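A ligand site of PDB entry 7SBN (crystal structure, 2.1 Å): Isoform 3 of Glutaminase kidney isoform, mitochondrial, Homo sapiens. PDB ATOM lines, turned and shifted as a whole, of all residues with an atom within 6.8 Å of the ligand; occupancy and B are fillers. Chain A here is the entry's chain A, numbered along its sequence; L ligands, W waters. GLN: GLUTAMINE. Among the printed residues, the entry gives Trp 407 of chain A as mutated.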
ATOM      1  N   TYR A 190     -12.344   7.708  -6.202  1.00  0.00           N
ATOM      2  CA  TYR A 190     -12.706   7.198  -7.524  1.00  0.00           C
ATOM      3  C   TYR A 190     -12.069   5.837  -7.807  1.00  0.00           C
ATOM      4  O   TYR A 190     -12.552   5.122  -8.694  1.00  0.00           O
ATOM      5  CB  TYR A 190     -12.341   8.220  -8.588  1.00  0.00           C
ATOM      6  CG  TYR A 190     -10.862   8.324  -8.900  1.00  0.00           C
ATOM      7  CD1 TYR A 190     -10.244   7.448  -9.812  1.00  0.00           C
ATOM      8  CD2 TYR A 190     -10.078   9.327  -8.316  1.00  0.00           C
ATOM      9  CE1 TYR A 190      -8.894   7.550 -10.109  1.00  0.00           C
ATOM     10  CE2 TYR A 190      -8.730   9.440  -8.612  1.00  0.00           C
ATOM     11  CZ  TYR A 190      -8.139   8.546  -9.504  1.00  0.00           C
ATOM     12  OH  TYR A 190      -6.796   8.667  -9.791  1.00  0.00           O
ATOM     13  N   ILE A 191     -11.014   5.461  -7.089  1.00  0.00           N
ATOM     14  CA  ILE A 191     -10.505   4.093  -7.109  1.00  0.00           C
ATOM     15  C   ILE A 191     -10.322   3.609  -5.673  1.00  0.00           C
ATOM     16  O   ILE A 191     -10.045   4.418  -4.768  1.00  0.00           O
ATOM     17  CB  ILE A 191      -9.193   3.962  -7.902  1.00  0.00           C
ATOM     18  CG1 ILE A 191      -8.177   5.025  -7.458  1.00  0.00           C
ATOM     19  CG2 ILE A 191      -9.471   4.043  -9.391  1.00  0.00           C
ATOM     20  CD1 ILE A 191      -6.817   4.861  -8.107  1.00  0.00           C
ATOM     21  N   LEU A 194      -6.927   4.600  -3.575  1.00  0.00           N
ATOM     22  CA  LEU A 194      -6.788   5.918  -2.976  1.00  0.00           C
ATOM     23  C   LEU A 194      -7.692   6.088  -1.773  1.00  0.00           C
ATOM     24  O   LEU A 194      -7.319   6.754  -0.806  1.00  0.00           O
ATOM     25  CB  LEU A 194      -7.054   7.021  -4.004  1.00  0.00           C
ATOM     26  CG  LEU A 194      -5.997   7.143  -5.102  1.00  0.00           C
ATOM     27  CD1 LEU A 194      -6.476   8.132  -6.140  1.00  0.00           C
ATOM     28  CD2 LEU A 194      -4.647   7.565  -4.563  1.00  0.00           C
ATOM     29  N   LEU A 225       2.472   9.091  -7.133  1.00  0.00           N
ATOM     30  CA  LEU A 225       2.696  10.456  -7.596  1.00  0.00           C
ATOM     31  C   LEU A 225       1.426  11.054  -8.188  1.00  0.00           C
ATOM     32  O   LEU A 225       1.148  12.248  -8.012  1.00  0.00           O
ATOM     33  CB  LEU A 225       3.827  10.471  -8.624  1.00  0.00           C
ATOM     34  CG  LEU A 225       5.261  10.490  -8.058  1.00  0.00           C
ATOM     35  CD1 LEU A 225       6.282  10.326  -9.172  1.00  0.00           C
ATOM     36  CD2 LEU A 225       5.522  11.773  -7.308  1.00  0.00           C
ATOM     37  N   GLN A 226       0.625  10.245  -8.895  1.00  0.00           N
ATOM     38  CA  GLN A 226      -0.541  10.739  -9.653  1.00  0.00           C
ATOM     39  C   GLN A 226      -0.085  11.943 -10.477  1.00  0.00           C
ATOM     40  O   GLN A 226       0.986  11.871 -11.096  1.00  0.00           O
ATOM     41  CB  GLN A 226      -1.711  10.984  -8.706  1.00  0.00           C
ATOM     42  CG  GLN A 226      -2.279   9.717  -8.084  1.00  0.00           C
ATOM     43  CD  GLN A 226      -3.015   8.828  -9.089  1.00  0.00           C
ATOM     44  OE1 GLN A 226      -3.275   9.235 -10.219  1.00  0.00           O
ATOM     45  NE2 GLN A 226      -3.369   7.619  -8.669  1.00  0.00           N
ATOM     46  N   SER A 227      -0.826  13.059 -10.500  1.00  0.00           N
ATOM     47  CA  SER A 227      -0.434  14.165 -11.382  1.00  0.00           C
ATOM     48  C   SER A 227       0.874  14.827 -10.959  1.00  0.00           C
ATOM     49  O   SER A 227       1.432  15.592 -11.753  1.00  0.00           O
ATOM     50  CB  SER A 227      -1.540  15.203 -11.469  1.00  0.00           C
ATOM     51  OG  SER A 227      -2.605  14.714 -12.284  1.00  0.00           O
ATOM     52  N   CYS A 228       1.390  14.544  -9.770  1.00  0.00           N
ATOM     53  CA  CYS A 228       2.710  15.057  -9.425  1.00  0.00           C
ATOM     54  C   CYS A 228       3.774  14.591 -10.418  1.00  0.00           C
ATOM     55  O   CYS A 228       4.853  15.198 -10.479  1.00  0.00           O
ATOM     56  CB  CYS A 228       3.106  14.605  -8.010  1.00  0.00           C
ATOM     57  SG  CYS A 228       2.104  15.273  -6.667  1.00  0.00           S
ATOM     58  N   LYS A 230       3.445  14.701 -13.617  1.00  0.00           N
ATOM     59  CA  LYS A 230       3.337  15.487 -14.848  1.00  0.00           C
ATOM     60  C   LYS A 230       4.523  16.423 -15.088  1.00  0.00           C
ATOM     61  O   LYS A 230       5.059  16.418 -16.219  1.00  0.00           O
ATOM     62  CB  LYS A 230       2.011  16.252 -14.837  1.00  0.00           C
ATOM     63  CG  LYS A 230       0.777  15.354 -14.957  1.00  0.00           C
ATOM     64  CD  LYS A 230      -0.489  16.180 -15.153  1.00  0.00           C
ATOM     65  CE  LYS A 230      -1.689  15.329 -15.621  1.00  0.00           C
ATOM     66  NZ  LYS A 230      -1.954  14.142 -14.786  1.00  0.00           N
ATOM     67  N   ASN A 276      -4.435  16.798 -17.800  1.00  0.00           N
ATOM     68  CA  ASN A 276      -4.463  15.411 -18.278  1.00  0.00           C
ATOM     69  C   ASN A 276      -4.201  15.327 -19.773  1.00  0.00           C
ATOM     70  O   ASN A 276      -3.422  14.490 -20.240  1.00  0.00           O
ATOM     71  CB  ASN A 276      -5.802  14.754 -17.935  1.00  0.00           C
ATOM     72  CG  ASN A 276      -5.925  14.420 -16.459  1.00  0.00           C
ATOM     73  OD1 ASN A 276      -5.264  15.037 -15.623  1.00  0.00           O
ATOM     74  ND2 ASN A 276      -6.741  13.419 -16.138  1.00  0.00           N
ATOM     75  N   ILE A 280      -1.003  13.484 -21.335  1.00  0.00           N
ATOM     76  CA  ILE A 280      -1.165  12.322 -22.206  1.00  0.00           C
ATOM     77  C   ILE A 280      -0.374  12.527 -23.483  1.00  0.00           C
ATOM     78  O   ILE A 280       0.264  11.594 -23.984  1.00  0.00           O
ATOM     79  CB  ILE A 280      -2.668  12.051 -22.462  1.00  0.00           C
ATOM     80  CG1 ILE A 280      -3.323  11.457 -21.211  1.00  0.00           C
ATOM     81  CG2 ILE A 280      -2.863  11.083 -23.634  1.00  0.00           C
ATOM     82  CD1 ILE A 280      -4.845  11.465 -21.259  1.00  0.00           C
ATOM     83  N   GLU A 322      -7.017   2.518 -12.066  1.00  0.00           N
ATOM     84  CA  GLU A 322      -7.014   3.683 -12.951  1.00  0.00           C
ATOM     85  C   GLU A 322      -7.489   3.322 -14.353  1.00  0.00           C
ATOM     86  O   GLU A 322      -8.252   4.066 -14.968  1.00  0.00           O
ATOM     87  CB  GLU A 322      -5.622   4.306 -13.029  1.00  0.00           C
ATOM     88  CG  GLU A 322      -5.139   4.961 -11.761  1.00  0.00           C
ATOM     89  CD  GLU A 322      -5.566   6.419 -11.666  1.00  0.00           C
ATOM     90  OE1 GLU A 322      -5.658   6.925 -10.530  1.00  0.00           O
ATOM     91  OE2 GLU A 322      -5.799   7.057 -12.726  1.00  0.00           O
ATOM     92  N   ARG A 328     -12.917   9.479 -18.345  1.00  0.00           N
ATOM     93  CA  ARG A 328     -12.546  10.808 -18.820  1.00  0.00           C
ATOM     94  C   ARG A 328     -11.235  10.779 -19.590  1.00  0.00           C
ATOM     95  O   ARG A 328     -11.093  11.487 -20.605  1.00  0.00           O
ATOM     96  CB  ARG A 328     -12.462  11.789 -17.657  1.00  0.00           C
ATOM     97  CG  ARG A 328     -12.378  13.223 -18.144  1.00  0.00           C
ATOM     98  CD  ARG A 328     -12.227  14.253 -17.035  1.00  0.00           C
ATOM     99  NE  ARG A 328     -11.913  15.580 -17.586  1.00  0.00           N
ATOM    100  CZ  ARG A 328     -10.754  16.212 -17.430  1.00  0.00           C
ATOM    101  NH1 ARG A 328      -9.772  15.643 -16.720  1.00  0.00           N
ATOM    102  NH2 ARG A 328     -10.564  17.405 -17.980  1.00  0.00           N
ATOM    103  N   ASN A 329     -10.268   9.955 -19.153  1.00  0.00           N
ATOM    104  CA  ASN A 329      -8.993   9.885 -19.867  1.00  0.00           C
ATOM    105  C   ASN A 329      -9.137   9.181 -21.203  1.00  0.00           C
ATOM    106  O   ASN A 329      -8.463   9.546 -22.183  1.00  0.00           O
ATOM    107  CB  ASN A 329      -7.937   9.206 -18.979  1.00  0.00           C
ATOM    108  CG  ASN A 329      -7.475  10.127 -17.839  1.00  0.00           C
ATOM    109  OD1 ASN A 329      -7.266  11.317 -18.058  1.00  0.00           O
ATOM    110  ND2 ASN A 329      -7.365   9.589 -16.620  1.00  0.00           N
ATOM    111  N   TYR A 355       0.347   6.132 -19.653  1.00  0.00           N
ATOM    112  CA  TYR A 355      -0.028   7.255 -18.801  1.00  0.00           C
ATOM    113  C   TYR A 355      -0.545   6.775 -17.440  1.00  0.00           C
ATOM    114  O   TYR A 355      -0.149   7.301 -16.394  1.00  0.00           O
ATOM    115  CB  TYR A 355      -1.077   8.137 -19.500  1.00  0.00           C
ATOM    116  CG  TYR A 355      -1.772   9.159 -18.589  1.00  0.00           C
ATOM    117  CD1 TYR A 355      -1.220  10.433 -18.375  1.00  0.00           C
ATOM    118  CD2 TYR A 355      -2.991   8.875 -17.972  1.00  0.00           C
ATOM    119  CE1 TYR A 355      -1.872  11.376 -17.554  1.00  0.00           C
ATOM    120  CE2 TYR A 355      -3.665   9.823 -17.181  1.00  0.00           C
ATOM    121  CZ  TYR A 355      -3.085  11.062 -16.960  1.00  0.00           C
ATOM    122  OH  TYR A 355      -3.725  11.988 -16.158  1.00  0.00           O
ATOM    123  N   PHE A 356      -1.426   5.765 -17.437  1.00  0.00           N
ATOM    124  CA  PHE A 356      -1.910   5.214 -16.169  1.00  0.00           C
ATOM    125  C   PHE A 356      -0.761   4.662 -15.338  1.00  0.00           C
ATOM    126  O   PHE A 356      -0.776   4.763 -14.102  1.00  0.00           O
ATOM    127  CB  PHE A 356      -2.948   4.119 -16.409  1.00  0.00           C
ATOM    128  CG  PHE A 356      -4.196   4.591 -17.115  1.00  0.00           C
ATOM    129  CD1 PHE A 356      -4.777   5.779 -16.766  1.00  0.00           C
ATOM    130  CD2 PHE A 356      -4.783   3.822 -18.123  1.00  0.00           C
ATOM    131  CE1 PHE A 356      -5.934   6.241 -17.416  1.00  0.00           C
ATOM    132  CE2 PHE A 356      -5.927   4.267 -18.771  1.00  0.00           C
ATOM    133  CZ  PHE A 356      -6.498   5.498 -18.413  1.00  0.00           C
ATOM    134  N   CYS A 359       1.160   7.566 -13.635  1.00  0.00           N
ATOM    135  CA  CYS A 359       0.402   8.094 -12.506  1.00  0.00           C
ATOM    136  C   CYS A 359       0.520   7.207 -11.272  1.00  0.00           C
ATOM    137  O   CYS A 359       0.359   7.696 -10.143  1.00  0.00           O
ATOM    138  CB  CYS A 359      -1.085   8.242 -12.879  1.00  0.00           C
ATOM    139  SG  CYS A 359      -1.436   9.494 -14.138  1.00  0.00           S
ATOM    140  N   SER A 360       0.769   5.914 -11.481  1.00  0.00           N
ATOM    141  CA  SER A 360       0.816   4.901 -10.430  1.00  0.00           C
ATOM    142  C   SER A 360       2.208   4.724  -9.838  1.00  0.00           C
ATOM    143  O   SER A 360       2.399   3.844  -8.995  1.00  0.00           O
ATOM    144  CB  SER A 360       0.319   3.555 -10.976  1.00  0.00           C
ATOM    145  OG  SER A 360      -1.040   3.641 -11.329  1.00  0.00           O
ATOM    146  N   TRP A 407      -4.184  22.937 -10.564  1.00  0.00           N
ATOM    147  CA  TRP A 407      -5.510  22.914 -11.176  1.00  0.00           C
ATOM    148  C   TRP A 407      -6.155  24.300 -11.184  1.00  0.00           C
ATOM    149  O   TRP A 407      -5.488  25.305 -11.443  1.00  0.00           O
ATOM    150  CB  TRP A 407      -6.408  21.892 -10.458  1.00  0.00           C
ATOM    151  CG  TRP A 407      -5.788  20.531 -10.457  1.00  0.00           C
ATOM    152  CD1 TRP A 407      -5.266  19.850  -9.376  1.00  0.00           C
ATOM    153  CD2 TRP A 407      -5.564  19.696 -11.591  1.00  0.00           C
ATOM    154  NE1 TRP A 407      -4.760  18.645  -9.778  1.00  0.00           N
ATOM    155  CE2 TRP A 407      -4.921  18.525 -11.138  1.00  0.00           C
ATOM    156  CE3 TRP A 407      -5.858  19.811 -12.953  1.00  0.00           C
ATOM    157  CZ2 TRP A 407      -4.571  17.478 -12.001  1.00  0.00           C
ATOM    158  CZ3 TRP A 407      -5.510  18.775 -13.816  1.00  0.00           C
ATOM    159  CH2 TRP A 407      -4.875  17.611 -13.322  1.00  0.00           C
ATOM    160  N   LYS A 422       3.153  21.337  -7.761  1.00  0.00           N
ATOM    161  CA  LYS A 422       2.316  20.439  -8.547  1.00  0.00           C
ATOM    162  C   LYS A 422       1.634  19.486  -7.586  1.00  0.00           C
ATOM    163  O   LYS A 422       2.319  18.731  -6.884  1.00  0.00           O
ATOM    164  CB  LYS A 422       3.114  19.652  -9.595  1.00  0.00           C
ATOM    165  CG  LYS A 422       2.203  18.779 -10.482  1.00  0.00           C
ATOM    166  CD  LYS A 422       1.331  19.628 -11.429  1.00  0.00           C
ATOM    167  CE  LYS A 422       0.068  18.885 -11.887  1.00  0.00           C
ATOM    168  NZ  LYS A 422      -1.083  19.042 -10.910  1.00  0.00           N
ATOM    169  N   SER A 423       0.304  19.529  -7.556  1.00  0.00           N
ATOM    170  CA  SER A 423      -0.468  18.638  -6.709  1.00  0.00           C
ATOM    171  C   SER A 423      -0.878  17.360  -7.451  1.00  0.00           C
ATOM    172  O   SER A 423      -0.908  17.311  -8.687  1.00  0.00           O
ATOM    173  CB  SER A 423      -1.721  19.348  -6.202  1.00  0.00           C
ATOM    174  OG  SER A 423      -2.536  19.689  -7.317  1.00  0.00           O
ATOM    175  N   GLY A 424      -1.241  16.345  -6.666  1.00  0.00           N
ATOM    176  CA  GLY A 424      -1.770  15.115  -7.200  1.00  0.00           C
ATOM    177  C   GLY A 424      -2.858  14.568  -6.294  1.00  0.00           C
ATOM    178  O   GLY A 424      -2.931  14.903  -5.107  1.00  0.00           O
ATOM    179  N   VAL A 425      -3.702  13.715  -6.873  1.00  0.00           N
ATOM    180  CA  VAL A 425      -4.943  13.311  -6.214  1.00  0.00           C
ATOM    181  C   VAL A 425      -4.726  12.358  -5.046  1.00  0.00           C
ATOM    182  O   VAL A 425      -5.632  12.156  -4.213  1.00  0.00           O
ATOM    183  CB  VAL A 425      -5.903  12.709  -7.271  1.00  0.00           C
ATOM    184  CG1 VAL A 425      -5.465  11.312  -7.667  1.00  0.00           C
ATOM    185  CG2 VAL A 425      -7.323  12.708  -6.784  1.00  0.00           C
ATOM    186  N   ALA A 426      -3.542  11.761  -4.941  1.00  0.00           N
ATOM    187  CA  ALA A 426      -3.182  11.027  -3.735  1.00  0.00           C
ATOM    188  C   ALA A 426      -2.866  11.952  -2.565  1.00  0.00           C
ATOM    189  O   ALA A 426      -2.663  11.450  -1.457  1.00  0.00           O
ATOM    190  CB  ALA A 426      -1.972  10.126  -4.002  1.00  0.00           C
ATOM    191  N   LEU A 446      -8.290  15.979   0.157  1.00  0.00           N
ATOM    192  CA  LEU A 446      -8.247  17.034  -0.843  1.00  0.00           C
ATOM    193  C   LEU A 446      -9.383  18.027  -0.646  1.00  0.00           C
ATOM    194  O   LEU A 446     -10.469  17.686  -0.157  1.00  0.00           O
ATOM    195  CB  LEU A 446      -8.325  16.452  -2.248  1.00  0.00           C
ATOM    196  CG  LEU A 446      -7.482  15.215  -2.588  1.00  0.00           C
ATOM    197  CD1 LEU A 446      -7.711  14.833  -4.038  1.00  0.00           C
ATOM    198  CD2 LEU A 446      -5.979  15.445  -2.336  1.00  0.00           C
ATOM    199  N   GLY A 450      -9.131  19.644  -5.705  1.00  0.00           N
ATOM    200  CA  GLY A 450      -8.227  18.522  -5.911  1.00  0.00           C
ATOM    201  C   GLY A 450      -6.869  18.655  -5.252  1.00  0.00           C
ATOM    202  O   GLY A 450      -5.981  17.830  -5.536  1.00  0.00           O
HETATM  203  N   GLN L   1      -4.831   9.423 -12.534  1.00  0.00           N
HETATM  204  CA  GLN L   1      -5.570  10.669 -12.369  1.00  0.00           C
HETATM  205  C   GLN L   1      -6.108  11.177 -13.713  1.00  0.00           C
HETATM  206  O   GLN L   1      -7.129  11.854 -13.746  1.00  0.00           O
HETATM  207  CB  GLN L   1      -4.688  11.746 -11.716  1.00  0.00           C
HETATM  208  CG  GLN L   1      -5.426  13.017 -11.300  1.00  0.00           C
HETATM  209  CD  GLN L   1      -4.639  13.877 -10.321  1.00  0.00           C
HETATM  210  OE1 GLN L   1      -3.666  13.422  -9.709  1.00  0.00           O
HETATM  211  NE2 GLN L   1      -5.063  15.118 -10.165  1.00  0.00           N
HETATM  212  OXT GLN L   1      -5.524  10.945 -14.777  1.00  0.00           O
HETATM  213  O   HOH W   1      -4.610  16.835  -7.531  1.00  0.00           O
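OH of Tyr 355 lies within hydrogen-bond range of OXT of the ligand (2.5 Å). The side-chain carboxylate of Glu 322 is in salt-bridge range of a nitrogen (N) of the ligand (2.6 Å). OE1 of Gln 226 sits at hydrogen-bond distance from N of the ligand. The backbone NH of Val 425 sits at hydrogen-bond distance from an oxygen (OE1) of the ligand, at 2.9 Å. The side-chain amide nitrogen (ND2) of Asn 276 sits at hydrogen-bond distance from an oxygen (O) of the ligand, at 2.9 Å. ND2 of Asn 329 lies within hydrogen-bond range of OXT of the ligand (2.9 Å). N of Ser 227 sits at hydrogen-bond distance from OE1 of the ligand, at 3.0 Å. An oxygen (OE1) of the ligand sits close to the side-chain hydroxyl (OG) of Ser 227 (3.1 Å). A nitrogen (N) of the ligand is in hydrogen-bond range of the side-chain hydroxyl (OH) of Tyr 190 (3.5 Å). The side-chain sulfur of Cys 359 lies within hydrogen-bond range of a nitrogen (N) of the ligand, 3.8 Å away.
O of Tyr 355 lies within hydrogen-bond range of SG of Cys 359, at 3.4 Å. The side-chain hydroxyl of Tyr 355 lies within hydrogen-bond range of the side-chain amino group of Lys 230 (3.1 Å). OE1 of Glu 322 is in hydrogen-bond range of NE2 of Gln 226, 3.0 Å away. The side-chain carboxylate of Glu 322 sits close to the side-chain hydroxyl of Tyr 190 (3.5 Å). ND2 of Asn 276 sits at hydrogen-bond distance from OD1 of Asn 329, 2.9 Å away. OG of Ser 227 lies within hydrogen-bond range of NZ of Lys 230 (2.6 Å). The side-chain hydroxyl of Ser 423 lies close to the indole nitrogen of Trp 407, at 3.5 Å. The side-chain sulfur of Cys 228 sits at hydrogen-bond distance from the backbone NH of Gly 424 (3.5 Å).
Residues that only touch the ligand: Trp 407 and Gly 424. Hydrophobic or aromatic side chains that line the ligand: Tyr 355, Trp 407 and Val 425. Within 4 Å of the ligand: Tyr 190, Gln 226, Ser 227, Asn 276, Glu 322, Asn 329, Tyr 355, Cys 359, Trp 407, Gly 424 and Val 425. The nearest printed residue that does not touch the ligand is Lys 230 (4.8 Å).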
